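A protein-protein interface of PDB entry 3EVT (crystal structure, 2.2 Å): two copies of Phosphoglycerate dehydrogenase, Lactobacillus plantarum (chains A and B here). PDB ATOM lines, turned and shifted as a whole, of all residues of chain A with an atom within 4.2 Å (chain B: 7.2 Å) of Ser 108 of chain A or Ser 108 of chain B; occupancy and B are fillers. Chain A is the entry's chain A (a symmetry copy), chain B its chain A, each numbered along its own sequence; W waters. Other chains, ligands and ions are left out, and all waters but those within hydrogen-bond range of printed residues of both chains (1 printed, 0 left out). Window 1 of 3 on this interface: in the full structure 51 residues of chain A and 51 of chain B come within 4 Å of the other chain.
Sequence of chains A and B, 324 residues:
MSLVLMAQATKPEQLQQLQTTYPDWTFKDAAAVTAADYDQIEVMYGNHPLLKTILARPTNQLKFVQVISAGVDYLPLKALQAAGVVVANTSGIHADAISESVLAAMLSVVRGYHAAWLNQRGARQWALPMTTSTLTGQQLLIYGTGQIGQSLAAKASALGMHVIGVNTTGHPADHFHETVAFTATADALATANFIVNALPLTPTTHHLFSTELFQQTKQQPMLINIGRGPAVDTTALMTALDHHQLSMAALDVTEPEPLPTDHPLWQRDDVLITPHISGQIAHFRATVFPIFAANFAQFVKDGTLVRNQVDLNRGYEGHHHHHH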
ATOM      1  N   ALA A 104      -7.918  25.190   5.402  1.00  0.00           N
ATOM      2  CA  ALA A 104      -8.034  25.134   6.844  1.00  0.00           C
ATOM      3  C   ALA A 104      -8.222  26.522   7.406  1.00  0.00           C
ATOM      4  O   ALA A 104      -9.046  26.741   8.315  1.00  0.00           O
ATOM      5  CB  ALA A 104      -6.765  24.470   7.450  1.00  0.00           C
ATOM      6  N   ALA A 105      -7.460  27.476   6.876  1.00  0.00           N
ATOM      7  CA  ALA A 105      -7.575  28.830   7.338  1.00  0.00           C
ATOM      8  C   ALA A 105      -8.987  29.355   7.033  1.00  0.00           C
ATOM      9  O   ALA A 105      -9.611  30.001   7.872  1.00  0.00           O
ATOM     10  CB  ALA A 105      -6.490  29.695   6.666  1.00  0.00           C
ATOM     11  N   MET A 106      -9.469  29.084   5.822  1.00  0.00           N
ATOM     12  CA  MET A 106     -10.720  29.631   5.328  1.00  0.00           C
ATOM     13  C   MET A 106     -11.880  28.975   6.052  1.00  0.00           C
ATOM     14  O   MET A 106     -12.796  29.660   6.504  1.00  0.00           O
ATOM     15  CB  MET A 106     -10.872  29.427   3.781  1.00  0.00           C
ATOM     16  CG  MET A 106      -9.901  30.220   2.854  1.00  0.00           C
ATOM     17  SD  MET A 106     -10.301  30.144   1.060  1.00  0.00           S
ATOM     18  CE  MET A 106     -10.101  28.430   0.699  1.00  0.00           C
ATOM     19  N   LEU A 107     -11.868  27.649   6.139  1.00  0.00           N
ATOM     20  CA  LEU A 107     -12.936  26.893   6.856  1.00  0.00           C
ATOM     21  C   LEU A 107     -13.013  27.165   8.352  1.00  0.00           C
ATOM     22  O   LEU A 107     -14.107  27.318   8.926  1.00  0.00           O
ATOM     23  CB  LEU A 107     -12.782  25.390   6.625  1.00  0.00           C
ATOM     24  CG  LEU A 107     -13.265  24.973   5.240  1.00  0.00           C
ATOM     25  CD1 LEU A 107     -12.609  23.598   4.773  1.00  0.00           C
ATOM     26  CD2 LEU A 107     -14.782  24.920   5.236  1.00  0.00           C
ATOM     27  N   SER A 108     -11.870  27.248   9.017  1.00  0.00           N
ATOM     28  CA  SER A 108     -11.963  27.484  10.438  1.00  0.00           C
ATOM     29  C   SER A 108     -12.558  28.839  10.762  1.00  0.00           C
ATOM     30  O   SER A 108     -13.245  28.952  11.752  1.00  0.00           O
ATOM     31  CB  SER A 108     -10.639  27.295  11.155  1.00  0.00           C
ATOM     32  OG  SER A 108      -9.744  28.304  10.833  1.00  0.00           O
ATOM     33  N   VAL A 109     -12.331  29.833   9.898  1.00  0.00           N
ATOM     34  CA  VAL A 109     -13.003  31.128   9.969  1.00  0.00           C
ATOM     35  C   VAL A 109     -14.478  31.072   9.620  1.00  0.00           C
ATOM     36  O   VAL A 109     -15.266  31.336  10.497  1.00  0.00           O
ATOM     37  CB  VAL A 109     -12.287  32.210   9.156  1.00  0.00           C
ATOM     38  CG1 VAL A 109     -13.243  33.436   8.879  1.00  0.00           C
ATOM     39  CG2 VAL A 109     -11.017  32.640   9.909  1.00  0.00           C
ATOM     40  N   VAL A 110     -14.864  30.679   8.396  1.00  0.00           N
ATOM     41  CA  VAL A 110     -16.289  30.775   8.011  1.00  0.00           C
ATOM     42  C   VAL A 110     -17.191  29.771   8.717  1.00  0.00           C
ATOM     43  O   VAL A 110     -18.384  30.034   8.885  1.00  0.00           O
ATOM     44  CB  VAL A 110     -16.573  30.722   6.480  1.00  0.00           C
ATOM     45  CG1 VAL A 110     -15.819  31.794   5.782  1.00  0.00           C
ATOM     46  CG2 VAL A 110     -16.260  29.322   5.908  1.00  0.00           C
ATOM     47  N   GLY A 112     -16.761  28.987  11.765  1.00  0.00           N
ATOM     48  CA  GLY A 112     -16.887  29.494  13.138  1.00  0.00           C
ATOM     49  C   GLY A 112     -15.983  28.888  14.195  1.00  0.00           C
ATOM     50  O   GLY A 112     -16.165  29.156  15.409  1.00  0.00           O
ATOM     51  N   TYR A 113     -14.984  28.100  13.782  1.00  0.00           N
ATOM     52  CA  TYR A 113     -14.072  27.478  14.735  1.00  0.00           C
ATOM     53  C   TYR A 113     -13.231  28.506  15.419  1.00  0.00           C
ATOM     54  O   TYR A 113     -13.077  28.449  16.624  1.00  0.00           O
ATOM     55  CB  TYR A 113     -13.268  26.310  14.090  1.00  0.00           C
ATOM     56  CG  TYR A 113     -14.111  25.035  14.170  1.00  0.00           C
ATOM     57  CD1 TYR A 113     -15.019  24.714  13.167  1.00  0.00           C
ATOM     58  CD2 TYR A 113     -14.078  24.237  15.313  1.00  0.00           C
ATOM     59  CE1 TYR A 113     -15.812  23.659  13.284  1.00  0.00           C
ATOM     60  CE2 TYR A 113     -14.858  23.174  15.434  1.00  0.00           C
ATOM     61  CZ  TYR A 113     -15.747  22.889  14.435  1.00  0.00           C
ATOM     62  OH  TYR A 113     -16.561  21.790  14.576  1.00  0.00           O
ATOM     63  N   HIS A 114     -12.736  29.503  14.692  1.00  0.00           N
ATOM     64  CA  HIS A 114     -11.934  30.516  15.332  1.00  0.00           C
ATOM     65  C   HIS A 114     -12.795  31.322  16.320  1.00  0.00           C
ATOM     66  O   HIS A 114     -12.408  31.510  17.494  1.00  0.00           O
ATOM     67  CB  HIS A 114     -11.308  31.454  14.298  1.00  0.00           C
ATOM     68  CG  HIS A 114     -10.517  32.557  14.912  1.00  0.00           C
ATOM     69  ND1 HIS A 114      -9.368  32.325  15.640  1.00  0.00           N
ATOM     70  CD2 HIS A 114     -10.726  33.898  14.945  1.00  0.00           C
ATOM     71  CE1 HIS A 114      -8.891  33.479  16.076  1.00  0.00           C
ATOM     72  NE2 HIS A 114      -9.692  34.450  15.661  1.00  0.00           N
ATOM     73  N   GLU B 100     -19.012  20.890   5.545  1.00  0.00           N
ATOM     74  CA  GLU B 100     -17.952  21.914   5.672  1.00  0.00           C
ATOM     75  C   GLU B 100     -17.491  22.142   7.127  1.00  0.00           C
ATOM     76  O   GLU B 100     -16.299  22.271   7.395  1.00  0.00           O
ATOM     77  CB  GLU B 100     -18.408  23.247   5.052  1.00  0.00           C
ATOM     78  CG  GLU B 100     -18.467  23.199   3.494  1.00  0.00           C
ATOM     79  CD  GLU B 100     -18.498  24.597   2.905  1.00  0.00           C
ATOM     80  OE1 GLU B 100     -18.124  25.550   3.664  1.00  0.00           O
ATOM     81  OE2 GLU B 100     -18.856  24.732   1.695  1.00  0.00           O
ATOM     82  N   VAL B 102     -17.527  19.838   9.491  1.00  0.00           N
ATOM     83  CA  VAL B 102     -16.663  18.695   9.860  1.00  0.00           C
ATOM     84  C   VAL B 102     -15.261  18.860   9.239  1.00  0.00           C
ATOM     85  O   VAL B 102     -14.234  18.657   9.902  1.00  0.00           O
ATOM     86  CB  VAL B 102     -17.288  17.363   9.467  1.00  0.00           C
ATOM     87  CG1 VAL B 102     -16.320  16.191   9.820  1.00  0.00           C
ATOM     88  CG2 VAL B 102     -18.634  17.203  10.199  1.00  0.00           C
ATOM     89  N   LEU B 103     -15.199  19.233   7.971  1.00  0.00           N
ATOM     90  CA  LEU B 103     -13.889  19.403   7.320  1.00  0.00           C
ATOM     91  C   LEU B 103     -13.085  20.456   8.096  1.00  0.00           C
ATOM     92  O   LEU B 103     -11.866  20.324   8.264  1.00  0.00           O
ATOM     93  CB  LEU B 103     -14.053  19.809   5.844  1.00  0.00           C
ATOM     94  CG  LEU B 103     -14.761  18.856   4.852  1.00  0.00           C
ATOM     95  CD1 LEU B 103     -14.939  19.588   3.518  1.00  0.00           C
ATOM     96  CD2 LEU B 103     -13.969  17.555   4.638  1.00  0.00           C
ATOM     97  N   ALA B 104     -13.787  21.494   8.570  1.00  0.00           N
ATOM     98  CA  ALA B 104     -13.189  22.615   9.264  1.00  0.00           C
ATOM     99  C   ALA B 104     -12.581  22.158  10.567  1.00  0.00           C
ATOM    100  O   ALA B 104     -11.468  22.579  10.938  1.00  0.00           O
ATOM    101  CB  ALA B 104     -14.264  23.710   9.520  1.00  0.00           C
ATOM    102  N   ALA B 105     -13.302  21.296  11.278  1.00  0.00           N
ATOM    103  CA  ALA B 105     -12.802  20.796  12.527  1.00  0.00           C
ATOM    104  C   ALA B 105     -11.515  19.993  12.276  1.00  0.00           C
ATOM    105  O   ALA B 105     -10.536  20.132  13.008  1.00  0.00           O
ATOM    106  CB  ALA B 105     -13.885  19.934  13.206  1.00  0.00           C
ATOM    107  N   MET B 106     -11.537  19.147  11.249  1.00  0.00           N
ATOM    108  CA  MET B 106     -10.461  18.214  10.970  1.00  0.00           C
ATOM    109  C   MET B 106      -9.254  18.973  10.454  1.00  0.00           C
ATOM    110  O   MET B 106      -8.134  18.739  10.905  1.00  0.00           O
ATOM    111  CB  MET B 106     -10.892  17.125   9.928  1.00  0.00           C
ATOM    112  CG  MET B 106     -11.971  16.092  10.374  1.00  0.00           C
ATOM    113  SD  MET B 106     -12.237  14.692   9.211  1.00  0.00           S
ATOM    114  CE  MET B 106     -12.843  15.505   7.770  1.00  0.00           C
ATOM    115  N   LEU B 107      -9.464  19.860   9.486  1.00  0.00           N
ATOM    116  CA  LEU B 107      -8.361  20.692   8.922  1.00  0.00           C
ATOM    117  C   LEU B 107      -7.725  21.660   9.909  1.00  0.00           C
ATOM    118  O   LEU B 107      -6.491  21.817   9.956  1.00  0.00           O
ATOM    119  CB  LEU B 107      -8.844  21.468   7.697  1.00  0.00           C
ATOM    120  CG  LEU B 107      -8.951  20.578   6.462  1.00  0.00           C
ATOM    121  CD1 LEU B 107      -9.955  21.180   5.383  1.00  0.00           C
ATOM    122  CD2 LEU B 107      -7.563  20.344   5.894  1.00  0.00           C
ATOM    123  N   SER B 108      -8.534  22.317  10.727  1.00  0.00           N
ATOM    124  CA  SER B 108      -7.915  23.247  11.642  1.00  0.00           C
ATOM    125  C   SER B 108      -7.019  22.558  12.650  1.00  0.00           C
ATOM    126  O   SER B 108      -6.023  23.129  13.032  1.00  0.00           O
ATOM    127  CB  SER B 108      -8.919  24.144  12.341  1.00  0.00           C
ATOM    128  OG  SER B 108      -9.681  23.429  13.253  1.00  0.00           O
ATOM    129  N   VAL B 109      -7.356  21.320  13.027  1.00  0.00           N
ATOM    130  CA  VAL B 109      -6.488  20.460  13.827  1.00  0.00           C
ATOM    131  C   VAL B 109      -5.258  19.972  13.085  1.00  0.00           C
ATOM    132  O   VAL B 109      -4.183  20.346  13.487  1.00  0.00           O
ATOM    133  CB  VAL B 109      -7.242  19.292  14.469  1.00  0.00           C
ATOM    134  CG1 VAL B 109      -6.244  18.159  14.930  1.00  0.00           C
ATOM    135  CG2 VAL B 109      -8.078  19.825  15.644  1.00  0.00           C
ATOM    136  N   VAL B 110      -5.395  19.207  11.990  1.00  0.00           N
ATOM    137  CA  VAL B 110      -4.199  18.605  11.362  1.00  0.00           C
ATOM    138  C   VAL B 110      -3.296  19.610  10.659  1.00  0.00           C
ATOM    139  O   VAL B 110      -2.093  19.371  10.537  1.00  0.00           O
ATOM    140  CB  VAL B 110      -4.477  17.413  10.398  1.00  0.00           C
ATOM    141  CG1 VAL B 110      -5.228  16.346  11.108  1.00  0.00           C
ATOM    142  CG2 VAL B 110      -5.205  17.891   9.124  1.00  0.00           C
ATOM    143  N   ARG B 111      -3.856  20.722  10.168  1.00  0.00           N
ATOM    144  CA  ARG B 111      -2.987  21.763   9.552  1.00  0.00           C
ATOM    145  C   ARG B 111      -2.439  22.744  10.571  1.00  0.00           C
ATOM    146  O   ARG B 111      -1.673  23.662  10.222  1.00  0.00           O
ATOM    147  CB  ARG B 111      -3.660  22.469   8.360  1.00  0.00           C
ATOM    148  CG  ARG B 111      -4.220  21.477   7.304  1.00  0.00           C
ATOM    149  CD  ARG B 111      -3.115  20.511   6.801  1.00  0.00           C
ATOM    150  NE  ARG B 111      -1.987  21.213   6.245  1.00  0.00           N
ATOM    151  CZ  ARG B 111      -0.739  20.738   6.274  1.00  0.00           C
ATOM    152  NH1 ARG B 111      -0.475  19.566   6.858  1.00  0.00           N
ATOM    153  NH2 ARG B 111       0.245  21.434   5.720  1.00  0.00           N
ATOM    154  N   GLY B 112      -2.771  22.509  11.847  1.00  0.00           N
ATOM    155  CA  GLY B 112      -2.091  23.229  12.931  1.00  0.00           C
ATOM    156  C   GLY B 112      -2.663  24.571  13.349  1.00  0.00           C
ATOM    157  O   GLY B 112      -2.028  25.307  14.145  1.00  0.00           O
ATOM    158  N   TYR B 113      -3.864  24.913  12.867  1.00  0.00           N
ATOM    159  CA  TYR B 113      -4.481  26.186  13.219  1.00  0.00           C
ATOM    160  C   TYR B 113      -4.841  26.223  14.668  1.00  0.00           C
ATOM    161  O   TYR B 113      -4.576  27.210  15.327  1.00  0.00           O
ATOM    162  CB  TYR B 113      -5.648  26.550  12.253  1.00  0.00           C
ATOM    163  CG  TYR B 113      -5.065  27.252  11.025  1.00  0.00           C
ATOM    164  CD1 TYR B 113      -4.631  26.521   9.923  1.00  0.00           C
ATOM    165  CD2 TYR B 113      -4.837  28.627  11.039  1.00  0.00           C
ATOM    166  CE1 TYR B 113      -4.042  27.124   8.901  1.00  0.00           C
ATOM    167  CE2 TYR B 113      -4.260  29.241  10.017  1.00  0.00           C
ATOM    168  CZ  TYR B 113      -3.836  28.495   8.952  1.00  0.00           C
ATOM    169  OH  TYR B 113      -3.227  29.140   7.902  1.00  0.00           O
ATOM    170  N   HIS B 114      -5.377  25.136  15.214  1.00  0.00           N
ATOM    171  CA  HIS B 114      -5.719  25.142  16.615  1.00  0.00           C
ATOM    172  C   HIS B 114      -4.444  25.254  17.468  1.00  0.00           C
ATOM    173  O   HIS B 114      -4.361  26.107  18.377  1.00  0.00           O
ATOM    174  CB  HIS B 114      -6.493  23.878  16.996  1.00  0.00           C
ATOM    175  CG  HIS B 114      -6.819  23.806  18.448  1.00  0.00           C
ATOM    176  ND1 HIS B 114      -7.665  24.707  19.059  1.00  0.00           N
ATOM    177  CD2 HIS B 114      -6.382  22.968  19.423  1.00  0.00           C
ATOM    178  CE1 HIS B 114      -7.754  24.413  20.346  1.00  0.00           C
ATOM    179  NE2 HIS B 114      -6.992  23.357  20.591  1.00  0.00           N
ATOM    180  N   ALA B 115      -3.452  24.402  17.209  1.00  0.00           N
ATOM    181  CA  ALA B 115      -2.168  24.569  17.912  1.00  0.00           C
ATOM    182  C   ALA B 115      -1.529  25.947  17.697  1.00  0.00           C
ATOM    183  O   ALA B 115      -0.965  26.516  18.634  1.00  0.00           O
ATOM    184  CB  ALA B 115      -1.149  23.434  17.543  1.00  0.00           C
ATOM    185  N   ALA B 116      -1.551  26.467  16.467  1.00  0.00           N
ATOM    186  CA  ALA B 116      -1.019  27.819  16.186  1.00  0.00           C
ATOM    187  C   ALA B 116      -1.682  28.895  17.013  1.00  0.00           C
ATOM    188  O   ALA B 116      -1.012  29.810  17.468  1.00  0.00           O
ATOM    189  CB  ALA B 116      -1.101  28.175  14.738  1.00  0.00           C
ATOM    190  N   MET B 130       3.791  20.398  17.679  1.00  0.00           N
ATOM    191  CA  MET B 130       3.032  19.316  17.114  1.00  0.00           C
ATOM    192  C   MET B 130       3.539  19.104  15.713  1.00  0.00           C
ATOM    193  O   MET B 130       4.192  19.978  15.154  1.00  0.00           O
ATOM    194  CB  MET B 130       1.501  19.619  17.190  1.00  0.00           C
ATOM    195  CG  MET B 130       1.016  20.956  16.569  1.00  0.00           C
ATOM    196  SD  MET B 130       0.801  20.940  14.751  1.00  0.00           S
ATOM    197  CE  MET B 130      -0.697  19.905  14.748  1.00  0.00           C
ATOM    198  N   MET B 222      -9.357  11.392  16.034  1.00  0.00           N
ATOM    199  CA  MET B 222     -10.070  12.568  16.494  1.00  0.00           C
ATOM    200  C   MET B 222     -11.598  12.231  16.457  1.00  0.00           C
ATOM    201  O   MET B 222     -12.095  11.616  15.494  1.00  0.00           O
ATOM    202  CB  MET B 222      -9.700  13.763  15.588  1.00  0.00           C
ATOM    203  CG  MET B 222     -10.484  15.077  15.840  1.00  0.00           C
ATOM    204  SD  MET B 222     -10.020  16.460  14.761  1.00  0.00           S
ATOM    205  CE  MET B 222     -11.082  17.672  15.547  1.00  0.00           C
ATOM    206  N   LEU B 272     -12.916  20.976  21.066  1.00  0.00           N
ATOM    207  CA  LEU B 272     -13.355  22.242  20.473  1.00  0.00           C
ATOM    208  C   LEU B 272     -14.843  22.274  20.555  1.00  0.00           C
ATOM    209  O   LEU B 272     -15.483  21.525  19.854  1.00  0.00           O
ATOM    210  CB  LEU B 272     -12.977  22.338  18.982  1.00  0.00           C
ATOM    211  CG  LEU B 272     -11.561  21.959  18.512  1.00  0.00           C
ATOM    212  CD1 LEU B 272     -11.320  22.118  16.974  1.00  0.00           C
ATOM    213  CD2 LEU B 272     -10.545  22.711  19.298  1.00  0.00           C
HETATM  214  O   HOH W   1     -17.207  21.500  17.362  1.00  0.00           O
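O of Ala 104 of chain B is in hydrogen-bond range of OG of Ser 108 of chain B (3.0 Å).
The side-chain hydroxyl (OG) of Ser 108 of chain B is in hydrogen-bond range of the backbone carbonyl oxygen (O) of Ala 105 of chain B, 3.4 Å away.
The backbone carbonyl oxygen of Ser 108 of chain B sits at hydrogen-bond distance from the backbone NH of Tyr 113 of chain B (2.8 Å).
The backbone carbonyl oxygen (O) of Ala 105 of chain A sits at hydrogen-bond distance from the side-chain hydroxyl (OG) of Ser 108 of chain A.
O of Ser 108 of chain A is in hydrogen-bond range of N of Tyr 113 of chain A (2.8 Å).
O of Ser 108 of chain A sits at hydrogen-bond distance from N of His 114 of chain A (3.0 Å).
Leu 107 of chain B touches Ala 104 of chain A (O to CB, 3.7 Å).
Ala 104 of chain A touches Arg 111 of chain B.
CD1 of Tyr 113 of chain B touches CB of Ala 104 of chain A, at 3.9 Å.
Ala 105 of chain A touches Tyr 113 of chain B (CB to OH, 3.5 Å).
Leu 107 of chain A touches Glu 100 of chain B (CD2 to O, 3.7 Å).
Leu 107 of chain A touches Ala 104 of chain B.
CD1 of Leu 107 of chain A touches CD1 of Leu 107 of chain B (3.6 Å).
CB of Ser 108 of chain B touches CB of Ser 108 of chain A, at 3.8 Å.
Ala 105 of chain B touches Tyr 113 of chain A (CB to OH, 3.5 Å).
Tyr 113 of chain A touches Leu 272 of chain B (CD2 to CD1, 3.9 Å).
Printed residues of chain A within 4 Å of Tyr 113 of chain B: Ala 104 and Ala 105.
Of the printed residues of chain A, Arg 111 of chain B touches Ala 104 (3.8 Å).
Of the printed residues of chain B, Tyr 113 of chain A touches Ala 104 (3.9 Å), Ala 105 (3.5 Å) and Leu 272 (3.9 Å).
Printed residues of chain B within 4 Å of Leu 107 of chain A: Glu 100, Ala 104 and Leu 107.
The nearest residue of chain B that does not touch Ser 108 of chain A is Ala 104 of chain B (4.3 Å).
The nearest printed residue of chain A that does not touch Ser 108 of chain B is Ala 104 of chain A (4.3 Å).
The nearest printed residue of chain B that does not touch Ala 105 of chain A is Leu 107 of chain B (6.2 Å).
Hydrophobic or aromatic side chains of chain B that line the printed part of chain A: Ala 104, Ala 105, Leu 107, Tyr 113 and Leu 272.
Along chain B the printed residues that touch a printed residue of chain A span positions 100 to 272.
Printed residues of chain A that touch a printed residue of chain B: Ala 104, Ala 105, Leu 107, Ser 108 and Tyr 113.
Hydrophobic or aromatic side chains of chain A that line the printed part of chain B: Ala 104, Ala 105, Leu 107 and Tyr 113.
Among the printed residues, 11 pairs touch across the chains.
Among the printed residues, no Asp or Glu carboxylate lies within 4 Å of a Lys or Arg side-chain nitrogen of the other chain.
Ala 104 of chain A touches Leu 107 of chain B, and with the chains exchanged Leu 107 of chain A touches Ala 104 of chain B.
Ala 104 of chain A touches Tyr 113 of chain B, and with the chains exchanged Tyr 113 of chain A touches Ala 104 of chain B.
Ala 105 of chain A touches Tyr 113 of chain B, and with the chains exchanged Tyr 113 of chain A touches Ala 105 of chain B.
Ser 108 of chain B touches its own counterpart, Ser 108 of chain A.
Positions printed for both chains: 104, 105, 106, 107, 108, 109, 110, 112, 113 and 114.
Of the 11 pairs that touch across the chains among the printed residues, 8 have their exchanged pair printed and touching as well.
Water W1 lies within hydrogen-bond range of OH of Tyr 113 of chain A (2.9 Å) and O of Leu 272 of chain B (3.0 Å).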
